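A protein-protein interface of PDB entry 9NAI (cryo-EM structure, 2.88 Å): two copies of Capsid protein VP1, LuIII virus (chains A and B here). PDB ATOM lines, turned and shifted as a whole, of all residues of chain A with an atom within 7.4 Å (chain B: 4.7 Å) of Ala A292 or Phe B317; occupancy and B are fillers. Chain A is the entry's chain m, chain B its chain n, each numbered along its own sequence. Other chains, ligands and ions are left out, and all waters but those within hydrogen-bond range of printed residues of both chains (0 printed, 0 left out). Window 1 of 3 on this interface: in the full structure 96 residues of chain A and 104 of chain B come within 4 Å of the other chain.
The backbone carbonyl oxygen (O) of Asn A249 sits close to the guanidinium group (NE) of Arg A296 (3.3 Å). O of Ala A298 lies close to OD1 of Asn A249 (2.7 Å). The backbone carbonyl oxygen (O) of Arg A250 is in hydrogen-bond range of the guanidinium group (NH2) of Arg A296 (3.2 Å). NE2 of Gln A299 sits at hydrogen-bond distance from O of Gly A301 (3.0 Å). The side-chain amide nitrogen of Asn B308 is in hydrogen-bond range of the side-chain carboxylate of Glu B310, at 3.2 Å. The backbone NH (N) of Glu B310 lies within hydrogen-bond range of the backbone carbonyl oxygen (O) of Phe B317 (3.0 Å).
No position is printed for both chains. Of the 24 pairs that touch across the chains among the printed residues, none has its exchanged pair printed and touching as well.
Of the 23 printed residues of chain A, 13 touch a printed residue of chain B. Hydrophobic or aromatic side chains of chain A that line the printed part of chain B: Ala A292 and Phe A376. Of the 13 printed residues of chain B, 13 touch a printed residue of chain A. Hydrophobic or aromatic side chains of chain B within 4 Å of the printed part of chain A: Met B62, Phe B309, Pro B316, Phe B317 and Val B319. Among the printed residues, 24 pairs touch across the chains.
Asn A249 touches Phe B317. NH1 of Arg A250 touches CA of Gly B315, at 3.5 Å. Asp B65 touches Glu A291. CB of Ala A292 touches O of Ala B63, 3.5 Å away. O of Ala A292 touches CA of Phe B317, 3.4 Å away. OE1 of Gln A299 touches CG1 of Val B319, 3.3 Å away. C of Arg A370 touches O of Thr B311, 3.8 Å away. Phe B317 touches Arg A370. Phe A376 touches Met B62 (CE2 to SD, 3.7 Å). Asn B308 touches Phe A376 (OD1 to O, 3.9 Å).
Of chain B, only Ala B63, Asp B65, Pro B316, Phe B317 and Lys B318 come within 4 Å of Ala A292. Of the printed residues of chain A, Phe B317 touches Asn A249 (3.0 Å), Ala A292 (3.4 Å) and Arg A370 (3.0 Å). Printed residues of chain A within 4 Å of Ala B63: Thr A290, Ala A292 and Thr A293. Printed residues of chain B within 4 Å of Gly A369: Ser B312 (3.3 Å). Of the printed residues of chain A, Lys B318 touches Ala A292 (3.0 Å). Val A289 touches none of the printed residues of chain B. Val A300 touches none of the printed residues of chain B. The nearest printed residue of chain B that does not touch Thr A290 is Asp B65 (4.6 Å).
The side-chain carboxylate (OD2) of Asp B65 is in salt-bridge range of the guanidinium group (NH1) of Arg A250 (2.9 Å). NH1 of Arg A250 sits at hydrogen-bond distance from O of Pro B316, at 2.9 Å. The backbone carbonyl oxygen (O) of Ala B63 sits at hydrogen-bond distance from the side-chain hydroxyl (OG1) of Thr A290 (3.0 Å). The backbone carbonyl oxygen (O) of Asp B65 is in hydrogen-bond range of the backbone NH (N) of Ala A292 (3.4 Å). The backbone carbonyl oxygen (O) of Ala A292 lies within hydrogen-bond range of the backbone NH (N) of Lys B318, 3.0 Å away. NE2 of Gln A299 is in hydrogen-bond range of OE1 of Glu B310, at 3.0 Å. The backbone carbonyl oxygen of Asp A367 is in hydrogen-bond range of the side-chain hydroxyl of Ser B312 (2.8 Å). The backbone carbonyl oxygen of Gly A369 lies close to the side-chain hydroxyl of Ser B312 (3.5 Å). The guanidinium group of Arg A370 lies within salt-bridge range of the side-chain carboxylate of Glu B310 (2.9 Å). The backbone carbonyl oxygen (O) of Asn A374 sits at hydrogen-bond distance from the side-chain hydroxyl (OG1) of Thr B311 (2.9 Å). The backbone carbonyl oxygen (O) of Phe B309 is in hydrogen-bond range of the backbone NH (N) of Phe A376, 2.9 Å away.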
ATOM      1  N   THR A 248      30.675  22.767  24.905  1.00  0.00           N
ATOM      2  CA  THR A 248      29.444  23.221  25.524  1.00  0.00           C
ATOM      3  C   THR A 248      28.276  22.903  24.602  1.00  0.00           C
ATOM      4  O   THR A 248      28.453  22.450  23.472  1.00  0.00           O
ATOM      5  CB  THR A 248      29.563  24.713  25.829  1.00  0.00           C
ATOM      6  OG1 THR A 248      30.697  24.919  26.674  1.00  0.00           O
ATOM      7  CG2 THR A 248      28.368  25.249  26.558  1.00  0.00           C
ATOM      8  N   ASN A 249      27.059  23.168  25.067  1.00  0.00           N
ATOM      9  CA  ASN A 249      25.898  22.919  24.237  1.00  0.00           C
ATOM     10  C   ASN A 249      25.876  23.819  23.023  1.00  0.00           C
ATOM     11  O   ASN A 249      25.178  23.521  22.054  1.00  0.00           O
ATOM     12  CB  ASN A 249      24.620  23.108  25.038  1.00  0.00           C
ATOM     13  CG  ASN A 249      23.424  22.582  24.313  1.00  0.00           C
ATOM     14  OD1 ASN A 249      23.536  21.648  23.535  1.00  0.00           O
ATOM     15  ND2 ASN A 249      22.271  23.170  24.554  1.00  0.00           N
ATOM     16  N   ARG A 250      26.619  24.906  23.050  1.00  0.00           N
ATOM     17  CA  ARG A 250      26.667  25.808  21.922  1.00  0.00           C
ATOM     18  C   ARG A 250      27.827  25.489  20.992  1.00  0.00           C
ATOM     19  O   ARG A 250      27.949  26.105  19.934  1.00  0.00           O
ATOM     20  CB  ARG A 250      26.736  27.242  22.441  1.00  0.00           C
ATOM     21  CG  ARG A 250      26.629  28.308  21.404  1.00  0.00           C
ATOM     22  CD  ARG A 250      26.561  29.639  22.072  1.00  0.00           C
ATOM     23  NE  ARG A 250      26.453  30.715  21.107  1.00  0.00           N
ATOM     24  CZ  ARG A 250      26.204  31.969  21.442  1.00  0.00           C
ATOM     25  NH1 ARG A 250      26.037  32.288  22.712  1.00  0.00           N
ATOM     26  NH2 ARG A 250      26.126  32.903  20.510  1.00  0.00           N
ATOM     27  N   HIS A 251      28.668  24.530  21.354  1.00  0.00           N
ATOM     28  CA  HIS A 251      29.739  24.062  20.493  1.00  0.00           C
ATOM     29  C   HIS A 251      29.385  22.812  19.708  1.00  0.00           C
ATOM     30  O   HIS A 251      30.251  22.271  19.023  1.00  0.00           O
ATOM     31  CB  HIS A 251      30.994  23.794  21.307  1.00  0.00           C
ATOM     32  CG  HIS A 251      31.516  24.997  22.010  1.00  0.00           C
ATOM     33  ND1 HIS A 251      32.039  26.077  21.338  1.00  0.00           N
ATOM     34  CD2 HIS A 251      31.623  25.284  23.326  1.00  0.00           C
ATOM     35  CE1 HIS A 251      32.432  26.986  22.210  1.00  0.00           C
ATOM     36  NE2 HIS A 251      32.192  26.529  23.424  1.00  0.00           N
ATOM     37  N   THR A 281      15.465  25.582  13.951  1.00  0.00           N
ATOM     38  CA  THR A 281      15.213  26.161  15.257  1.00  0.00           C
ATOM     39  C   THR A 281      13.812  25.804  15.720  1.00  0.00           C
ATOM     40  O   THR A 281      12.938  25.485  14.912  1.00  0.00           O
ATOM     41  CB  THR A 281      15.370  27.673  15.242  1.00  0.00           C
ATOM     42  OG1 THR A 281      15.287  28.163  16.583  1.00  0.00           O
ATOM     43  CG2 THR A 281      14.275  28.302  14.423  1.00  0.00           C
ATOM     44  N   ARG A 286       9.387  33.595  13.909  1.00  0.00           N
ATOM     45  CA  ARG A 286      10.489  34.442  13.487  1.00  0.00           C
ATOM     46  C   ARG A 286      11.250  33.758  12.367  1.00  0.00           C
ATOM     47  O   ARG A 286      11.430  32.538  12.369  1.00  0.00           O
ATOM     48  CB  ARG A 286      11.433  34.755  14.637  1.00  0.00           C
ATOM     49  CG  ARG A 286      12.064  33.533  15.227  1.00  0.00           C
ATOM     50  CD  ARG A 286      13.503  33.770  15.614  1.00  0.00           C
ATOM     51  NE  ARG A 286      14.282  32.556  15.412  1.00  0.00           N
ATOM     52  CZ  ARG A 286      15.525  32.378  15.840  1.00  0.00           C
ATOM     53  NH1 ARG A 286      16.143  33.336  16.509  1.00  0.00           N
ATOM     54  NH2 ARG A 286      16.147  31.233  15.599  1.00  0.00           N
ATOM     55  N   VAL A 289      18.024  32.460  12.010  1.00  0.00           N
ATOM     56  CA  VAL A 289      18.809  31.370  12.562  1.00  0.00           C
ATOM     57  C   VAL A 289      19.980  32.007  13.279  1.00  0.00           C
ATOM     58  O   VAL A 289      20.777  32.712  12.656  1.00  0.00           O
ATOM     59  CB  VAL A 289      19.305  30.389  11.493  1.00  0.00           C
ATOM     60  CG1 VAL A 289      20.216  29.377  12.121  1.00  0.00           C
ATOM     61  CG2 VAL A 289      18.140  29.688  10.840  1.00  0.00           C
ATOM     62  N   THR A 290      20.084  31.780  14.573  1.00  0.00           N
ATOM     63  CA  THR A 290      21.186  32.330  15.331  1.00  0.00           C
ATOM     64  C   THR A 290      21.875  31.208  16.074  1.00  0.00           C
ATOM     65  O   THR A 290      21.261  30.204  16.438  1.00  0.00           O
ATOM     66  CB  THR A 290      20.720  33.388  16.316  1.00  0.00           C
ATOM     67  OG1 THR A 290      19.812  32.790  17.241  1.00  0.00           O
ATOM     68  CG2 THR A 290      20.005  34.484  15.578  1.00  0.00           C
ATOM     69  N   GLU A 291      23.170  31.397  16.291  1.00  0.00           N
ATOM     70  CA  GLU A 291      23.948  30.382  16.976  1.00  0.00           C
ATOM     71  C   GLU A 291      23.338  30.049  18.324  1.00  0.00           C
ATOM     72  O   GLU A 291      23.446  28.913  18.791  1.00  0.00           O
ATOM     73  CB  GLU A 291      25.383  30.867  17.136  1.00  0.00           C
ATOM     74  CG  GLU A 291      26.322  29.830  17.673  1.00  0.00           C
ATOM     75  CD  GLU A 291      26.538  28.700  16.694  1.00  0.00           C
ATOM     76  OE1 GLU A 291      26.178  28.858  15.510  1.00  0.00           O
ATOM     77  OE2 GLU A 291      27.063  27.648  17.108  1.00  0.00           O
ATOM     78  N   ALA A 292      22.677  31.016  18.949  1.00  0.00           N
ATOM     79  CA  ALA A 292      22.070  30.781  20.249  1.00  0.00           C
ATOM     80  C   ALA A 292      20.749  30.041  20.135  1.00  0.00           C
ATOM     81  O   ALA A 292      20.422  29.219  20.994  1.00  0.00           O
ATOM     82  CB  ALA A 292      21.867  32.102  20.977  1.00  0.00           C
ATOM     83  N   THR A 293      19.966  30.326  19.107  1.00  0.00           N
ATOM     84  CA  THR A 293      18.634  29.762  19.002  1.00  0.00           C
ATOM     85  C   THR A 293      18.567  28.507  18.155  1.00  0.00           C
ATOM     86  O   THR A 293      17.492  27.919  18.038  1.00  0.00           O
ATOM     87  CB  THR A 293      17.675  30.796  18.436  1.00  0.00           C
ATOM     88  OG1 THR A 293      18.151  31.222  17.158  1.00  0.00           O
ATOM     89  CG2 THR A 293      17.593  31.982  19.355  1.00  0.00           C
ATOM     90  N   ARG A 294      19.668  28.077  17.560  1.00  0.00           N
ATOM     91  CA  ARG A 294      19.611  26.902  16.710  1.00  0.00           C
ATOM     92  C   ARG A 294      19.486  25.643  17.547  1.00  0.00           C
ATOM     93  O   ARG A 294      19.986  25.562  18.669  1.00  0.00           O
ATOM     94  CB  ARG A 294      20.846  26.817  15.825  1.00  0.00           C
ATOM     95  CG  ARG A 294      22.115  26.731  16.602  1.00  0.00           C
ATOM     96  CD  ARG A 294      23.299  26.654  15.686  1.00  0.00           C
ATOM     97  NE  ARG A 294      23.317  25.415  14.928  1.00  0.00           N
ATOM     98  CZ  ARG A 294      24.226  25.137  14.005  1.00  0.00           C
ATOM     99  NH1 ARG A 294      25.179  26.012  13.736  1.00  0.00           N
ATOM    100  NH2 ARG A 294      24.186  23.985  13.361  1.00  0.00           N
ATOM    101  N   VAL A 295      18.803  24.651  16.986  1.00  0.00           N
ATOM    102  CA  VAL A 295      18.586  23.403  17.694  1.00  0.00           C
ATOM    103  C   VAL A 295      19.910  22.681  17.874  1.00  0.00           C
ATOM    104  O   VAL A 295      20.781  22.712  16.999  1.00  0.00           O
ATOM    105  CB  VAL A 295      17.579  22.536  16.929  1.00  0.00           C
ATOM    106  CG1 VAL A 295      17.437  21.197  17.583  1.00  0.00           C
ATOM    107  CG2 VAL A 295      16.250  23.222  16.890  1.00  0.00           C
ATOM    108  N   ARG A 296      20.068  22.038  19.015  1.00  0.00           N
ATOM    109  CA  ARG A 296      21.235  21.236  19.325  1.00  0.00           C
ATOM    110  C   ARG A 296      20.794  19.812  19.596  1.00  0.00           C
ATOM    111  O   ARG A 296      19.632  19.570  19.928  1.00  0.00           O
ATOM    112  CB  ARG A 296      21.957  21.796  20.549  1.00  0.00           C
ATOM    113  CG  ARG A 296      22.447  23.198  20.361  1.00  0.00           C
ATOM    114  CD  ARG A 296      23.528  23.276  19.324  1.00  0.00           C
ATOM    115  NE  ARG A 296      24.024  24.639  19.221  1.00  0.00           N
ATOM    116  CZ  ARG A 296      24.857  25.063  18.283  1.00  0.00           C
ATOM    117  NH1 ARG A 296      25.301  24.223  17.366  1.00  0.00           N
ATOM    118  NH2 ARG A 296      25.254  26.322  18.273  1.00  0.00           N
ATOM    119  N   ALA A 298      21.280  17.764  22.097  1.00  0.00           N
ATOM    120  CA  ALA A 298      20.835  17.478  23.451  1.00  0.00           C
ATOM    121  C   ALA A 298      21.256  18.620  24.357  1.00  0.00           C
ATOM    122  O   ALA A 298      22.090  19.446  23.997  1.00  0.00           O
ATOM    123  CB  ALA A 298      21.404  16.155  23.950  1.00  0.00           C
ATOM    124  N   GLN A 299      20.654  18.664  25.537  1.00  0.00           N
ATOM    125  CA  GLN A 299      21.057  19.605  26.571  1.00  0.00           C
ATOM    126  C   GLN A 299      22.287  19.072  27.287  1.00  0.00           C
ATOM    127  O   GLN A 299      22.274  17.945  27.789  1.00  0.00           O
ATOM    128  CB  GLN A 299      19.941  19.820  27.582  1.00  0.00           C
ATOM    129  CG  GLN A 299      20.288  20.857  28.605  1.00  0.00           C
ATOM    130  CD  GLN A 299      19.168  21.110  29.572  1.00  0.00           C
ATOM    131  OE1 GLN A 299      18.083  20.556  29.437  1.00  0.00           O
ATOM    132  NE2 GLN A 299      19.425  21.947  30.566  1.00  0.00           N
ATOM    133  N   VAL A 300      23.334  19.878  27.355  1.00  0.00           N
ATOM    134  CA  VAL A 300      24.546  19.516  28.073  1.00  0.00           C
ATOM    135  C   VAL A 300      24.535  20.233  29.408  1.00  0.00           C
ATOM    136  O   VAL A 300      24.569  21.466  29.461  1.00  0.00           O
ATOM    137  CB  VAL A 300      25.801  19.869  27.270  1.00  0.00           C
ATOM    138  CG1 VAL A 300      27.021  19.600  28.102  1.00  0.00           C
ATOM    139  CG2 VAL A 300      25.840  19.057  26.008  1.00  0.00           C
ATOM    140  N   GLY A 301      24.468  19.468  30.489  1.00  0.00           N
ATOM    141  CA  GLY A 301      24.323  20.038  31.808  1.00  0.00           C
ATOM    142  C   GLY A 301      22.931  20.599  31.986  1.00  0.00           C
ATOM    143  O   GLY A 301      22.165  20.752  31.040  1.00  0.00           O
ATOM    144  N   ASP A 367      32.328  22.056  30.175  1.00  0.00           N
ATOM    145  CA  ASP A 367      31.133  22.104  29.346  1.00  0.00           C
ATOM    146  C   ASP A 367      29.857  22.343  30.152  1.00  0.00           C
ATOM    147  O   ASP A 367      29.166  23.344  29.945  1.00  0.00           O
ATOM    148  CB  ASP A 367      31.051  20.818  28.530  1.00  0.00           C
ATOM    149  CG  ASP A 367      31.113  19.598  29.394  1.00  0.00           C
ATOM    150  OD1 ASP A 367      31.316  19.761  30.613  1.00  0.00           O
ATOM    151  OD2 ASP A 367      30.982  18.479  28.863  1.00  0.00           O
ATOM    152  N   GLY A 369      28.708  23.191  33.059  1.00  0.00           N
ATOM    153  CA  GLY A 369      28.393  24.140  34.107  1.00  0.00           C
ATOM    154  C   GLY A 369      27.275  25.092  33.723  1.00  0.00           C
ATOM    155  O   GLY A 369      26.868  25.198  32.569  1.00  0.00           O
ATOM    156  N   ARG A 370      26.757  25.794  34.729  1.00  0.00           N
ATOM    157  CA  ARG A 370      25.724  26.801  34.532  1.00  0.00           C
ATOM    158  C   ARG A 370      26.128  28.081  35.234  1.00  0.00           C
ATOM    159  O   ARG A 370      26.433  28.063  36.429  1.00  0.00           O
ATOM    160  CB  ARG A 370      24.377  26.353  35.080  1.00  0.00           C
ATOM    161  CG  ARG A 370      23.845  25.122  34.440  1.00  0.00           C
ATOM    162  CD  ARG A 370      23.607  25.381  32.996  1.00  0.00           C
ATOM    163  NE  ARG A 370      23.072  24.214  32.324  1.00  0.00           N
ATOM    164  CZ  ARG A 370      23.045  24.088  31.010  1.00  0.00           C
ATOM    165  NH1 ARG A 370      23.538  25.054  30.261  1.00  0.00           N
ATOM    166  NH2 ARG A 370      22.535  23.010  30.446  1.00  0.00           N
ATOM    167  N   ASN A 374      23.500  34.831  34.097  1.00  0.00           N
ATOM    168  CA  ASN A 374      23.257  34.986  32.679  1.00  0.00           C
ATOM    169  C   ASN A 374      22.193  34.045  32.135  1.00  0.00           C
ATOM    170  O   ASN A 374      21.948  34.052  30.930  1.00  0.00           O
ATOM    171  CB  ASN A 374      24.555  34.827  31.899  1.00  0.00           C
ATOM    172  CG  ASN A 374      25.495  35.981  32.125  1.00  0.00           C
ATOM    173  OD1 ASN A 374      25.081  37.039  32.587  1.00  0.00           O
ATOM    174  ND2 ASN A 374      26.748  35.814  31.740  1.00  0.00           N
ATOM    175  N   PHE A 376      18.263  33.013  31.613  1.00  0.00           N
ATOM    176  CA  PHE A 376      17.011  33.752  31.583  1.00  0.00           C
ATOM    177  C   PHE A 376      15.961  32.949  30.838  1.00  0.00           C
ATOM    178  O   PHE A 376      16.274  32.021  30.092  1.00  0.00           O
ATOM    179  CB  PHE A 376      17.188  35.120  30.933  1.00  0.00           C
ATOM    180  CG  PHE A 376      17.654  35.055  29.522  1.00  0.00           C
ATOM    181  CD1 PHE A 376      16.753  34.995  28.487  1.00  0.00           C
ATOM    182  CD2 PHE A 376      18.995  35.043  29.227  1.00  0.00           C
ATOM    183  CE1 PHE A 376      17.181  34.939  27.190  1.00  0.00           C
ATOM    184  CE2 PHE A 376      19.423  34.982  27.931  1.00  0.00           C
ATOM    185  CZ  PHE A 376      18.515  34.931  26.912  1.00  0.00           C
ATOM    186  N   MET B  62      20.212  39.515  23.115  1.00  0.00           N
ATOM    187  CA  MET B  62      20.983  38.352  23.512  1.00  0.00           C
ATOM    188  C   MET B  62      20.702  37.147  22.638  1.00  0.00           C
ATOM    189  O   MET B  62      21.620  36.413  22.268  1.00  0.00           O
ATOM    190  CB  MET B  62      20.597  38.015  24.936  1.00  0.00           C
ATOM    191  CG  MET B  62      20.896  39.105  25.892  1.00  0.00           C
ATOM    192  SD  MET B  62      20.214  38.601  27.447  1.00  0.00           S
ATOM    193  CE  MET B  62      18.493  38.881  27.083  1.00  0.00           C
ATOM    194  N   ALA B  63      19.437  36.943  22.290  1.00  0.00           N
ATOM    195  CA  ALA B  63      19.056  35.750  21.555  1.00  0.00           C
ATOM    196  C   ALA B  63      19.726  35.649  20.197  1.00  0.00           C
ATOM    197  O   ALA B  63      19.811  34.548  19.650  1.00  0.00           O
ATOM    198  CB  ALA B  63      17.544  35.705  21.378  1.00  0.00           C
ATOM    199  N   ASP B  65      22.917  36.427  19.496  1.00  0.00           N
ATOM    200  CA  ASP B  65      24.368  36.301  19.542  1.00  0.00           C
ATOM    201  C   ASP B  65      24.841  35.119  18.711  1.00  0.00           C
ATOM    202  O   ASP B  65      24.419  33.984  18.937  1.00  0.00           O
ATOM    203  CB  ASP B  65      24.821  36.131  20.987  1.00  0.00           C
ATOM    204  CG  ASP B  65      26.311  35.943  21.105  1.00  0.00           C
ATOM    205  OD1 ASP B  65      27.063  36.877  20.775  1.00  0.00           O
ATOM    206  OD2 ASP B  65      26.736  34.859  21.541  1.00  0.00           O
ATOM    207  N   ASN B 308      13.581  28.632  27.260  1.00  0.00           N
ATOM    208  CA  ASN B 308      14.564  28.612  28.327  1.00  0.00           C
ATOM    209  C   ASN B 308      15.952  28.811  27.739  1.00  0.00           C
ATOM    210  O   ASN B 308      16.396  28.019  26.904  1.00  0.00           O
ATOM    211  CB  ASN B 308      14.490  27.288  29.077  1.00  0.00           C
ATOM    212  CG  ASN B 308      15.375  27.263  30.283  1.00  0.00           C
ATOM    213  OD1 ASN B 308      15.647  28.295  30.887  1.00  0.00           O
ATOM    214  ND2 ASN B 308      15.834  26.077  30.652  1.00  0.00           N
ATOM    215  N   PHE B 309      16.633  29.863  28.173  1.00  0.00           N
ATOM    216  CA  PHE B 309      18.000  30.138  27.761  1.00  0.00           C
ATOM    217  C   PHE B 309      18.927  29.976  28.948  1.00  0.00           C
ATOM    218  O   PHE B 309      18.793  30.688  29.947  1.00  0.00           O
ATOM    219  CB  PHE B 309      18.125  31.536  27.173  1.00  0.00           C
ATOM    220  CG  PHE B 309      17.458  31.691  25.857  1.00  0.00           C
ATOM    221  CD1 PHE B 309      18.129  31.375  24.700  1.00  0.00           C
ATOM    222  CD2 PHE B 309      16.155  32.116  25.771  1.00  0.00           C
ATOM    223  CE1 PHE B 309      17.526  31.509  23.484  1.00  0.00           C
ATOM    224  CE2 PHE B 309      15.547  32.249  24.555  1.00  0.00           C
ATOM    225  CZ  PHE B 309      16.232  31.943  23.411  1.00  0.00           C
ATOM    226  N   GLU B 310      19.864  29.048  28.834  1.00  0.00           N
ATOM    227  CA  GLU B 310      20.862  28.807  29.857  1.00  0.00           C
ATOM    228  C   GLU B 310      22.236  29.126  29.296  1.00  0.00           C
ATOM    229  O   GLU B 310      22.471  29.011  28.093  1.00  0.00           O
ATOM    230  CB  GLU B 310      20.810  27.362  30.336  1.00  0.00           C
ATOM    231  CG  GLU B 310      19.514  27.022  31.027  1.00  0.00           C
ATOM    232  CD  GLU B 310      19.441  25.577  31.459  1.00  0.00           C
ATOM    233  OE1 GLU B 310      20.325  24.792  31.081  1.00  0.00           O
ATOM    234  OE2 GLU B 310      18.490  25.221  32.178  1.00  0.00           O
ATOM    235  N   THR B 311      23.142  29.534  30.174  1.00  0.00           N
ATOM    236  CA  THR B 311      24.437  30.048  29.756  1.00  0.00           C
ATOM    237  C   THR B 311      25.547  29.308  30.480  1.00  0.00           C
ATOM    238  O   THR B 311      25.673  29.407  31.703  1.00  0.00           O
ATOM    239  CB  THR B 311      24.533  31.541  30.026  1.00  0.00           C
ATOM    240  OG1 THR B 311      23.522  32.219  29.277  1.00  0.00           O
ATOM    241  CG2 THR B 311      25.882  32.052  29.610  1.00  0.00           C
ATOM    242  N   SER B 312      26.332  28.562  29.728  1.00  0.00           N
ATOM    243  CA  SER B 312      27.621  28.062  30.157  1.00  0.00           C
ATOM    244  C   SER B 312      28.711  28.975  29.610  1.00  0.00           C
ATOM    245  O   SER B 312      28.440  30.067  29.109  1.00  0.00           O
ATOM    246  CB  SER B 312      27.810  26.620  29.722  1.00  0.00           C
ATOM    247  OG  SER B 312      29.090  26.163  30.107  1.00  0.00           O
ATOM    248  N   GLY B 315      28.228  30.800  26.085  1.00  0.00           N
ATOM    249  CA  GLY B 315      27.293  31.879  25.919  1.00  0.00           C
ATOM    250  C   GLY B 315      25.881  31.405  26.152  1.00  0.00           C
ATOM    251  O   GLY B 315      25.644  30.280  26.590  1.00  0.00           O
ATOM    252  N   PRO B 316      24.911  32.258  25.868  1.00  0.00           N
ATOM    253  CA  PRO B 316      23.518  31.848  25.996  1.00  0.00           C
ATOM    254  C   PRO B 316      23.114  30.926  24.867  1.00  0.00           C
ATOM    255  O   PRO B 316      23.606  31.024  23.742  1.00  0.00           O
ATOM    256  CB  PRO B 316      22.762  33.174  25.913  1.00  0.00           C
ATOM    257  CG  PRO B 316      23.636  34.020  25.096  1.00  0.00           C
ATOM    258  CD  PRO B 316      25.031  33.665  25.474  1.00  0.00           C
ATOM    259  N   PHE B 317      22.215  30.005  25.187  1.00  0.00           N
ATOM    260  CA  PHE B 317      21.621  29.150  24.178  1.00  0.00           C
ATOM    261  C   PHE B 317      20.257  28.699  24.660  1.00  0.00           C
ATOM    262  O   PHE B 317      20.009  28.616  25.862  1.00  0.00           O
ATOM    263  CB  PHE B 317      22.489  27.937  23.881  1.00  0.00           C
ATOM    264  CG  PHE B 317      22.780  27.107  25.079  1.00  0.00           C
ATOM    265  CD1 PHE B 317      21.912  26.126  25.483  1.00  0.00           C
ATOM    266  CD2 PHE B 317      23.937  27.296  25.792  1.00  0.00           C
ATOM    267  CE1 PHE B 317      22.183  25.372  26.586  1.00  0.00           C
ATOM    268  CE2 PHE B 317      24.211  26.534  26.888  1.00  0.00           C
ATOM    269  CZ  PHE B 317      23.335  25.571  27.279  1.00  0.00           C
ATOM    270  N   LYS B 318      19.385  28.383  23.715  1.00  0.00           N
ATOM    271  CA  LYS B 318      18.067  27.884  24.061  1.00  0.00           C
ATOM    272  C   LYS B 318      18.133  26.407  24.397  1.00  0.00           C
ATOM    273  O   LYS B 318      18.738  25.622  23.667  1.00  0.00           O
ATOM    274  CB  LYS B 318      17.086  28.092  22.920  1.00  0.00           C
ATOM    275  CG  LYS B 318      15.721  27.590  23.280  1.00  0.00           C
ATOM    276  CD  LYS B 318      14.708  27.912  22.234  1.00  0.00           C
ATOM    277  CE  LYS B 318      13.378  27.325  22.620  1.00  0.00           C
ATOM    278  NZ  LYS B 318      13.415  25.849  22.509  1.00  0.00           N
ATOM    279  N   VAL B 319      17.497  26.027  25.491  1.00  0.00           N
ATOM    280  CA  VAL B 319      17.451  24.610  25.846  1.00  0.00           C
ATOM    281  C   VAL B 319      16.575  23.877  24.843  1.00  0.00           C
ATOM    282  O   VAL B 319      15.492  24.369  24.497  1.00  0.00           O
ATOM    283  CB  VAL B 319      16.919  24.438  27.258  1.00  0.00           C
ATOM    284  CG1 VAL B 319      16.769  22.975  27.582  1.00  0.00           C
ATOM    285  CG2 VAL B 319      17.848  25.098  28.236  1.00  0.00           C
